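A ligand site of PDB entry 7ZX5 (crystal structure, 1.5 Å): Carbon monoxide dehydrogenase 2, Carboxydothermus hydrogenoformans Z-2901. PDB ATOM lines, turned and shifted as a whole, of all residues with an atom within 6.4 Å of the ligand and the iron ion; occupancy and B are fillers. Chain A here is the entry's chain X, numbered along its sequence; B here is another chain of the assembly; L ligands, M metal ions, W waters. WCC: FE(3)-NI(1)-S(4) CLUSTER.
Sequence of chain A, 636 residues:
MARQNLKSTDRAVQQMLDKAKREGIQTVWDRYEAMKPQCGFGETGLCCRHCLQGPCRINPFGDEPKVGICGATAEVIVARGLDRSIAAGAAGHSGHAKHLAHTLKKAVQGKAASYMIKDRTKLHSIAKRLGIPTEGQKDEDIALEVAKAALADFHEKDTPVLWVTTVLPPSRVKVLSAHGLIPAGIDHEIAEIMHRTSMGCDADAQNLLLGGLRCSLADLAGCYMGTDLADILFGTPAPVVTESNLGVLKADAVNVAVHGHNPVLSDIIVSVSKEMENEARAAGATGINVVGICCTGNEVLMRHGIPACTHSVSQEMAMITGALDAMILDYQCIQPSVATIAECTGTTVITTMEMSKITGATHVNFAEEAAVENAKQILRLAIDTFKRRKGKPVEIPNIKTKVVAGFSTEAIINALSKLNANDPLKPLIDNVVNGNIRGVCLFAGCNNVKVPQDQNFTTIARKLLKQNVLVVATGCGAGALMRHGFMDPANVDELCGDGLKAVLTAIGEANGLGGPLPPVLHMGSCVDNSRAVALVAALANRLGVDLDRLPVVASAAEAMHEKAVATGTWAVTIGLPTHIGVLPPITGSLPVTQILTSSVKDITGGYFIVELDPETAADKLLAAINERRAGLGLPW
Water W1 lies within hydrogen-bond range of NZ of Lys 563 and SG of Cys 526.
Cys 526 touches the iron ion (CB to FE, 3.8 Å). Lys 563 touches the iron ion. The nearest printed residue that does not touch the iron ion is Cys 333 (4.4 Å).
O of Gln 332 sits close to ND1 of His 261 (3.2 Å). The side-chain sulfur (SG) of Cys 333 lies close to the side-chain amino group (NZ) of Lys 563, at 3.5 Å. The side-chain sulfur (SG) of Cys 446 sits close to the backbone NH (N) of Met 560. The backbone NH (N) of Cys 526 sits at hydrogen-bond distance from the side-chain sulfur (SG) of Cys 295. O of Gly 260 lies within hydrogen-bond range of N of Cys 295 (3.2 Å). A ring nitrogen (ND1) of His 561 is in hydrogen-bond range of the backbone NH (N) of Lys 563, at 2.9 Å. NZ of Lys 563 sits at hydrogen-bond distance from OE1 of Gln 332, at 2.8 Å. N of Ser 312 lies within hydrogen-bond range of SG of Cys 294 (3.4 Å).
O of Gly 445 sits close to S1 of the ligand (3.3 Å). Merely in contact with the ligand: Cys 526 (3.4 Å), Met 560 (3.7 Å) and His 561 (3.8 Å). Hydrophobic or aromatic side chains that line the ligand: His 261, Met 560 and His 561. Within 4 Å of the ligand: His 261, Cys 294, Cys 295, Ser 312, Cys 333, Gly 445, Cys 446, Cys 476, Cys 526, Met 560, His 561 and Lys 563. Along chain A the residues within 4 Å of the ligand span positions 261 to 563. The nearest printed residue that does not touch the ligand is Gly 475 (4.4 Å).
NE2 of His 261 is bound to the iron ion, 1.9 Å away. The iron ion is bound by water W1, 2.3 Å away. The iron ion is bound by S3 of the ligand, 2.5 Å away. The iron ion has three donor atoms within binding distance. Slightly farther from the iron ion lies SG of Cys 295 (3.0 Å).
An iron atom (FE1) of the ligand is bound by the side-chain sulfur of Cys 333, 2.2 Å away. The backbone NH (N) of Cys 476 sits close to a sulfur (S1) of the ligand (3.6 Å). The side-chain sulfur (SG) of Cys 476 binds an iron atom (FE4) of the ligand (2.4 Å). N of Cys 446 lies close to S1 of the ligand (3.6 Å). The side-chain sulfur (SG) of Cys 446 is bound to an iron atom (FE3) of the ligand, 2.5 Å away. A sulfur (S3) of the ligand lies close to the side-chain sulfur (SG) of Cys 295 (3.8 Å). NZ of Lys 563 lies close to S4 of the ligand, 3.5 Å away. A sulfur (S2) of the ligand sits close to the side-chain hydroxyl (OG) of Ser 312 (3.5 Å). A sulfur (S3) of the ligand sits close to the side-chain sulfur (SG) of Cys 294, at 3.7 Å.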
ATOM      1  N   HIS A  93      -2.248  17.490  28.272  1.00  0.00           N
ATOM      2  CA  HIS A  93      -3.640  17.075  28.213  1.00  0.00           C
ATOM      3  C   HIS A  93      -3.878  15.875  29.091  1.00  0.00           C
ATOM      4  O   HIS A  93      -4.924  15.774  29.740  1.00  0.00           O
ATOM      5  CB  HIS A  93      -4.033  16.736  26.805  1.00  0.00           C
ATOM      6  CG  HIS A  93      -4.338  17.932  25.960  1.00  0.00           C
ATOM      7  ND1 HIS A  93      -3.938  18.013  24.664  1.00  0.00           N
ATOM      8  CD2 HIS A  93      -4.993  19.101  26.222  1.00  0.00           C
ATOM      9  CE1 HIS A  93      -4.355  19.168  24.147  1.00  0.00           C
ATOM     10  NE2 HIS A  93      -4.958  19.853  25.084  1.00  0.00           N
ATOM     11  N   GLY A 260      -6.700  28.817  33.380  1.00  0.00           N
ATOM     12  CA  GLY A 260      -5.985  27.551  33.334  1.00  0.00           C
ATOM     13  C   GLY A 260      -6.783  26.533  32.561  1.00  0.00           C
ATOM     14  O   GLY A 260      -7.486  26.915  31.612  1.00  0.00           O
ATOM     15  N   HIS A 261      -6.772  25.273  33.043  1.00  0.00           N
ATOM     16  CA  HIS A 261      -7.455  24.186  32.322  1.00  0.00           C
ATOM     17  C   HIS A 261      -8.356  23.244  33.096  1.00  0.00           C
ATOM     18  O   HIS A 261      -9.348  22.789  32.528  1.00  0.00           O
ATOM     19  CB  HIS A 261      -6.484  23.359  31.635  1.00  0.00           C
ATOM     20  CG  HIS A 261      -5.982  24.045  30.440  1.00  0.00           C
ATOM     21  ND1 HIS A 261      -5.223  25.193  30.562  1.00  0.00           N
ATOM     22  CD2 HIS A 261      -6.256  23.899  29.130  1.00  0.00           C
ATOM     23  CE1 HIS A 261      -5.026  25.690  29.345  1.00  0.00           C
ATOM     24  NE2 HIS A 261      -5.631  24.916  28.476  1.00  0.00           N
ATOM     25  N   CYS A 294      -9.491  31.410  29.233  1.00  0.00           N
ATOM     26  CA  CYS A 294      -8.883  30.218  28.634  1.00  0.00           C
ATOM     27  C   CYS A 294      -9.799  29.002  28.905  1.00  0.00           C
ATOM     28  O   CYS A 294     -11.028  29.146  29.028  1.00  0.00           O
ATOM     29  CB  CYS A 294      -7.453  30.022  29.114  1.00  0.00           C
ATOM     30  SG  CYS A 294      -6.235  30.957  28.221  1.00  0.00           S
ATOM     31  N   CYS A 295      -9.229  27.815  29.038  1.00  0.00           N
ATOM     32  CA  CYS A 295     -10.107  26.648  28.938  1.00  0.00           C
ATOM     33  C   CYS A 295     -10.825  26.355  30.249  1.00  0.00           C
ATOM     34  O   CYS A 295     -11.992  25.902  30.214  1.00  0.00           O
ATOM     35  CB  CYS A 295      -9.329  25.463  28.379  1.00  0.00           C
ATOM     36  SG  CYS A 295      -9.331  25.551  26.611  1.00  0.00           S
ATOM     37  N   THR A 296     -10.244  26.642  31.413  1.00  0.00           N
ATOM     38  CA  THR A 296     -11.058  26.490  32.613  1.00  0.00           C
ATOM     39  C   THR A 296     -12.286  27.409  32.546  1.00  0.00           C
ATOM     40  O   THR A 296     -13.369  27.001  32.971  1.00  0.00           O
ATOM     41  CB  THR A 296     -10.208  26.713  33.871  1.00  0.00           C
ATOM     42  OG1 THR A 296     -10.693  25.832  34.909  1.00  0.00           O
ATOM     43  CG2 THR A 296     -10.245  28.168  34.321  1.00  0.00           C
ATOM     44  N   HIS A 311      -9.405  35.453  26.492  1.00  0.00           N
ATOM     45  CA  HIS A 311      -8.678  34.262  26.092  1.00  0.00           C
ATOM     46  C   HIS A 311      -7.217  34.496  25.691  1.00  0.00           C
ATOM     47  O   HIS A 311      -6.851  35.512  25.068  1.00  0.00           O
ATOM     48  CB  HIS A 311      -9.391  33.603  24.917  1.00  0.00           C
ATOM     49  CG  HIS A 311     -10.841  33.336  25.182  1.00  0.00           C
ATOM     50  ND1 HIS A 311     -11.843  34.241  24.864  1.00  0.00           N
ATOM     51  CD2 HIS A 311     -11.478  32.248  25.682  1.00  0.00           C
ATOM     52  CE1 HIS A 311     -13.012  33.727  25.198  1.00  0.00           C
ATOM     53  NE2 HIS A 311     -12.818  32.525  25.707  1.00  0.00           N
ATOM     54  N   SER A 312      -6.422  33.489  25.926  1.00  0.00           N
ATOM     55  CA  SER A 312      -5.133  33.292  25.303  1.00  0.00           C
ATOM     56  C   SER A 312      -4.253  34.536  25.358  1.00  0.00           C
ATOM     57  O   SER A 312      -3.967  35.125  26.423  1.00  0.00           O
ATOM     58  CB  SER A 312      -5.415  32.842  23.849  1.00  0.00           C
ATOM     59  OG  SER A 312      -4.307  32.310  23.226  1.00  0.00           O
ATOM     60  N   VAL A 313      -3.915  35.023  24.167  1.00  0.00           N
ATOM     61  CA  VAL A 313      -2.874  36.049  24.025  1.00  0.00           C
ATOM     62  C   VAL A 313      -3.276  37.350  24.784  1.00  0.00           C
ATOM     63  O   VAL A 313      -2.377  38.074  25.258  1.00  0.00           O
ATOM     64  CB  VAL A 313      -2.584  36.344  22.521  1.00  0.00           C
ATOM     65  CG1 VAL A 313      -3.806  37.063  21.851  1.00  0.00           C
ATOM     66  CG2 VAL A 313      -1.366  37.150  22.402  1.00  0.00           C
ATOM     67  N   GLN A 332      -1.324  25.552  32.710  1.00  0.00           N
ATOM     68  CA  GLN A 332      -1.307  25.631  31.263  1.00  0.00           C
ATOM     69  C   GLN A 332      -1.867  26.951  30.737  1.00  0.00           C
ATOM     70  O   GLN A 332      -2.975  27.394  31.093  1.00  0.00           O
ATOM     71  CB  GLN A 332      -2.034  24.440  30.611  1.00  0.00           C
ATOM     72  CG  GLN A 332      -1.450  23.039  30.914  1.00  0.00           C
ATOM     73  CD  GLN A 332      -2.430  21.917  30.531  1.00  0.00           C
ATOM     74  OE1 GLN A 332      -3.370  22.100  29.752  1.00  0.00           O
ATOM     75  NE2 GLN A 332      -2.249  20.755  31.140  1.00  0.00           N
ATOM     76  N   CYS A 333      -1.062  27.602  29.904  1.00  0.00           N
ATOM     77  CA  CYS A 333      -1.465  28.719  29.066  1.00  0.00           C
ATOM     78  C   CYS A 333      -1.638  30.009  29.832  1.00  0.00           C
ATOM     79  O   CYS A 333      -2.225  30.980  29.311  1.00  0.00           O
ATOM     80  CB  CYS A 333      -2.725  28.371  28.297  1.00  0.00           C
ATOM     81  SG  CYS A 333      -2.469  27.013  27.168  1.00  0.00           S
ATOM     82  N   ALA A 444      -9.897  25.169  16.314  1.00  0.00           N
ATOM     83  CA  ALA A 444      -9.302  24.675  17.541  1.00  0.00           C
ATOM     84  C   ALA A 444      -8.046  25.481  17.844  1.00  0.00           C
ATOM     85  O   ALA A 444      -7.509  26.187  16.995  1.00  0.00           O
ATOM     86  CB  ALA A 444      -8.927  23.196  17.462  1.00  0.00           C
ATOM     87  N   GLY A 445      -7.609  25.357  19.100  1.00  0.00           N
ATOM     88  CA  GLY A 445      -6.361  25.955  19.515  1.00  0.00           C
ATOM     89  C   GLY A 445      -6.420  27.408  19.917  1.00  0.00           C
ATOM     90  O   GLY A 445      -7.454  28.027  20.227  1.00  0.00           O
ATOM     91  N   CYS A 446      -5.235  27.977  19.852  1.00  0.00           N
ATOM     92  CA  CYS A 446      -4.876  29.172  20.562  1.00  0.00           C
ATOM     93  C   CYS A 446      -5.037  30.429  19.710  1.00  0.00           C
ATOM     94  O   CYS A 446      -5.329  30.345  18.528  1.00  0.00           O
ATOM     95  CB  CYS A 446      -3.391  29.009  20.955  1.00  0.00           C
ATOM     96  SG  CYS A 446      -2.747  27.272  21.294  1.00  0.00           S
ATOM     97  N   ASN A 447      -4.753  31.590  20.302  1.00  0.00           N
ATOM     98  CA  ASN A 447      -4.231  32.762  19.619  1.00  0.00           C
ATOM     99  C   ASN A 447      -2.696  32.749  19.690  1.00  0.00           C
ATOM    100  O   ASN A 447      -2.108  31.997  20.469  1.00  0.00           O
ATOM    101  CB  ASN A 447      -4.722  34.085  20.229  1.00  0.00           C
ATOM    102  CG  ASN A 447      -6.209  34.264  20.200  1.00  0.00           C
ATOM    103  OD1 ASN A 447      -6.800  34.637  21.250  1.00  0.00           O
ATOM    104  ND2 ASN A 447      -6.812  34.253  18.985  1.00  0.00           N
ATOM    105  N   THR A 474     -13.728  24.941  19.620  1.00  0.00           N
ATOM    106  CA  THR A 474     -13.309  24.694  20.963  1.00  0.00           C
ATOM    107  C   THR A 474     -12.201  25.657  21.393  1.00  0.00           C
ATOM    108  O   THR A 474     -11.594  26.333  20.591  1.00  0.00           O
ATOM    109  CB  THR A 474     -12.759  23.292  21.113  1.00  0.00           C
ATOM    110  OG1 THR A 474     -11.559  23.187  20.350  1.00  0.00           O
ATOM    111  CG2 THR A 474     -13.742  22.269  20.649  1.00  0.00           C
ATOM    112  N   GLY A 475     -11.933  25.639  22.691  1.00  0.00           N
ATOM    113  CA  GLY A 475     -10.772  26.328  23.210  1.00  0.00           C
ATOM    114  C   GLY A 475     -10.774  27.793  22.838  1.00  0.00           C
ATOM    115  O   GLY A 475     -11.787  28.459  22.869  1.00  0.00           O
ATOM    116  N   CYS A 476      -9.598  28.321  22.537  1.00  0.00           N
ATOM    117  CA  CYS A 476      -9.510  29.744  22.236  1.00  0.00           C
ATOM    118  C   CYS A 476      -9.931  30.055  20.799  1.00  0.00           C
ATOM    119  O   CYS A 476     -10.167  31.231  20.469  1.00  0.00           O
ATOM    120  CB  CYS A 476      -8.104  30.249  22.576  1.00  0.00           C
ATOM    121  SG  CYS A 476      -7.806  30.108  24.416  1.00  0.00           S
ATOM    122  N   GLY A 477     -10.162  29.022  19.962  1.00  0.00           N
ATOM    123  CA  GLY A 477     -10.903  29.241  18.717  1.00  0.00           C
ATOM    124  C   GLY A 477     -12.360  29.584  18.977  1.00  0.00           C
ATOM    125  O   GLY A 477     -12.902  30.558  18.444  1.00  0.00           O
ATOM    126  N   SER A 525     -13.943  23.097  25.801  1.00  0.00           N
ATOM    127  CA  SER A 525     -12.533  23.321  26.026  1.00  0.00           C
ATOM    128  C   SER A 525     -11.667  22.566  25.032  1.00  0.00           C
ATOM    129  O   SER A 525     -12.141  21.831  24.169  1.00  0.00           O
ATOM    130  CB  SER A 525     -12.199  22.817  27.403  1.00  0.00           C
ATOM    131  OG  SER A 525     -12.383  21.418  27.392  1.00  0.00           O
ATOM    132  N   CYS A 526     -10.323  22.764  25.118  1.00  0.00           N
ATOM    133  CA  CYS A 526      -9.420  22.032  24.248  1.00  0.00           C
ATOM    134  C   CYS A 526      -9.537  20.516  24.449  1.00  0.00           C
ATOM    135  O   CYS A 526      -9.554  19.764  23.469  1.00  0.00           O
ATOM    136  CB  CYS A 526      -7.972  22.479  24.467  1.00  0.00           C
ATOM    137  SG  CYS A 526      -6.830  21.778  23.255  1.00  0.00           S
ATOM    138  N   VAL A 527      -9.668  20.017  25.690  1.00  0.00           N
ATOM    139  CA  VAL A 527      -9.796  18.544  25.793  1.00  0.00           C
ATOM    140  C   VAL A 527     -11.096  18.107  25.101  1.00  0.00           C
ATOM    141  O   VAL A 527     -11.161  17.007  24.534  1.00  0.00           O
ATOM    142  CB  VAL A 527      -9.752  17.973  27.258  1.00  0.00           C
ATOM    143  CG1 VAL A 527      -8.368  18.113  27.808  1.00  0.00           C
ATOM    144  CG2 VAL A 527     -10.758  18.660  28.164  1.00  0.00           C
ATOM    145  N   MET A 560      -0.499  28.038  19.004  1.00  0.00           N
ATOM    146  CA  MET A 560       0.662  28.433  19.813  1.00  0.00           C
ATOM    147  C   MET A 560       1.283  27.285  20.654  1.00  0.00           C
ATOM    148  O   MET A 560       2.491  27.033  20.594  1.00  0.00           O
ATOM    149  CB  MET A 560       0.216  29.522  20.751  1.00  0.00           C
ATOM    150  CG  MET A 560       1.217  30.037  21.724  1.00  0.00           C
ATOM    151  SD  MET A 560       1.202  29.331  23.414  1.00  0.00           S
ATOM    152  CE  MET A 560      -0.439  29.635  23.946  1.00  0.00           C
ATOM    153  N   HIS A 561       0.455  26.640  21.428  1.00  0.00           N
ATOM    154  CA  HIS A 561       0.931  25.783  22.515  1.00  0.00           C
ATOM    155  C   HIS A 561       1.379  24.443  21.940  1.00  0.00           C
ATOM    156  O   HIS A 561       0.910  23.980  20.914  1.00  0.00           O
ATOM    157  CB  HIS A 561      -0.132  25.569  23.586  1.00  0.00           C
ATOM    158  CG  HIS A 561       0.390  25.048  24.888  1.00  0.00           C
ATOM    159  ND1 HIS A 561       0.741  23.727  25.119  1.00  0.00           N
ATOM    160  CD2 HIS A 561       0.647  25.718  26.037  1.00  0.00           C
ATOM    161  CE1 HIS A 561       1.214  23.627  26.343  1.00  0.00           C
ATOM    162  NE2 HIS A 561       1.113  24.798  26.940  1.00  0.00           N
ATOM    163  N   LYS A 563       0.466  21.694  23.054  1.00  0.00           N
ATOM    164  CA  LYS A 563      -0.838  21.016  23.028  1.00  0.00           C
ATOM    165  C   LYS A 563      -1.533  21.140  21.673  1.00  0.00           C
ATOM    166  O   LYS A 563      -2.147  20.156  21.201  1.00  0.00           O
ATOM    167  CB  LYS A 563      -1.766  21.559  24.112  1.00  0.00           C
ATOM    168  CG  LYS A 563      -1.428  21.063  25.485  1.00  0.00           C
ATOM    169  CD  LYS A 563      -2.281  21.654  26.621  1.00  0.00           C
ATOM    170  CE  LYS A 563      -2.037  23.092  26.852  1.00  0.00           C
ATOM    171  NZ  LYS A 563      -3.326  23.652  27.415  1.00  0.00           N
ATOM    172  N   ALA A 564      -1.498  22.327  21.093  1.00  0.00           N
ATOM    173  CA  ALA A 564      -2.100  22.544  19.772  1.00  0.00           C
ATOM    174  C   ALA A 564      -1.375  21.729  18.678  1.00  0.00           C
ATOM    175  O   ALA A 564      -2.002  21.167  17.762  1.00  0.00           O
ATOM    176  CB  ALA A 564      -2.091  24.039  19.416  1.00  0.00           C
ATOM    177  N   MET B 199       4.448  25.638  27.941  1.00  0.00           N
ATOM    178  CA  MET B 199       4.145  27.038  28.054  1.00  0.00           C
ATOM    179  C   MET B 199       3.007  27.308  29.055  1.00  0.00           C
ATOM    180  O   MET B 199       1.938  26.636  29.069  1.00  0.00           O
ATOM    181  CB  MET B 199       3.798  27.554  26.662  1.00  0.00           C
ATOM    182  CG  MET B 199       3.460  29.009  26.606  1.00  0.00           C
ATOM    183  SD  MET B 199       1.763  29.323  27.028  1.00  0.00           S
ATOM    184  CE  MET B 199       1.510  31.093  26.676  1.00  0.00           C
HETATM  185 NI   WCC L   1      -5.702  24.918  23.965  1.00  0.00          NI
HETATM  186 FE1  WCC L   1      -4.079  27.252  25.756  1.00  0.00          FE
HETATM  187 FE3  WCC L   1      -4.248  27.155  23.267  1.00  0.00          FE
HETATM  188 FE4  WCC L   1      -6.201  28.403  24.661  1.00  0.00          FE
HETATM  189  S1  WCC L   1      -6.362  26.772  23.088  1.00  0.00           S
HETATM  190  S2  WCC L   1      -4.026  29.008  24.451  1.00  0.00           S
HETATM  191  S3  WCC L   1      -6.163  27.556  26.731  1.00  0.00           S
HETATM  192  S4  WCC L   1      -3.775  25.494  24.495  1.00  0.00           S
HETATM  193 FE    FE M   1      -6.404  25.094  26.766  1.00  0.00          FE
HETATM  194  O   HOH W   1      -5.397  23.302  25.693  1.00  0.00           O
HETATM  195  O   HOH W   2      -4.035  24.338  22.157  1.00  0.00           O
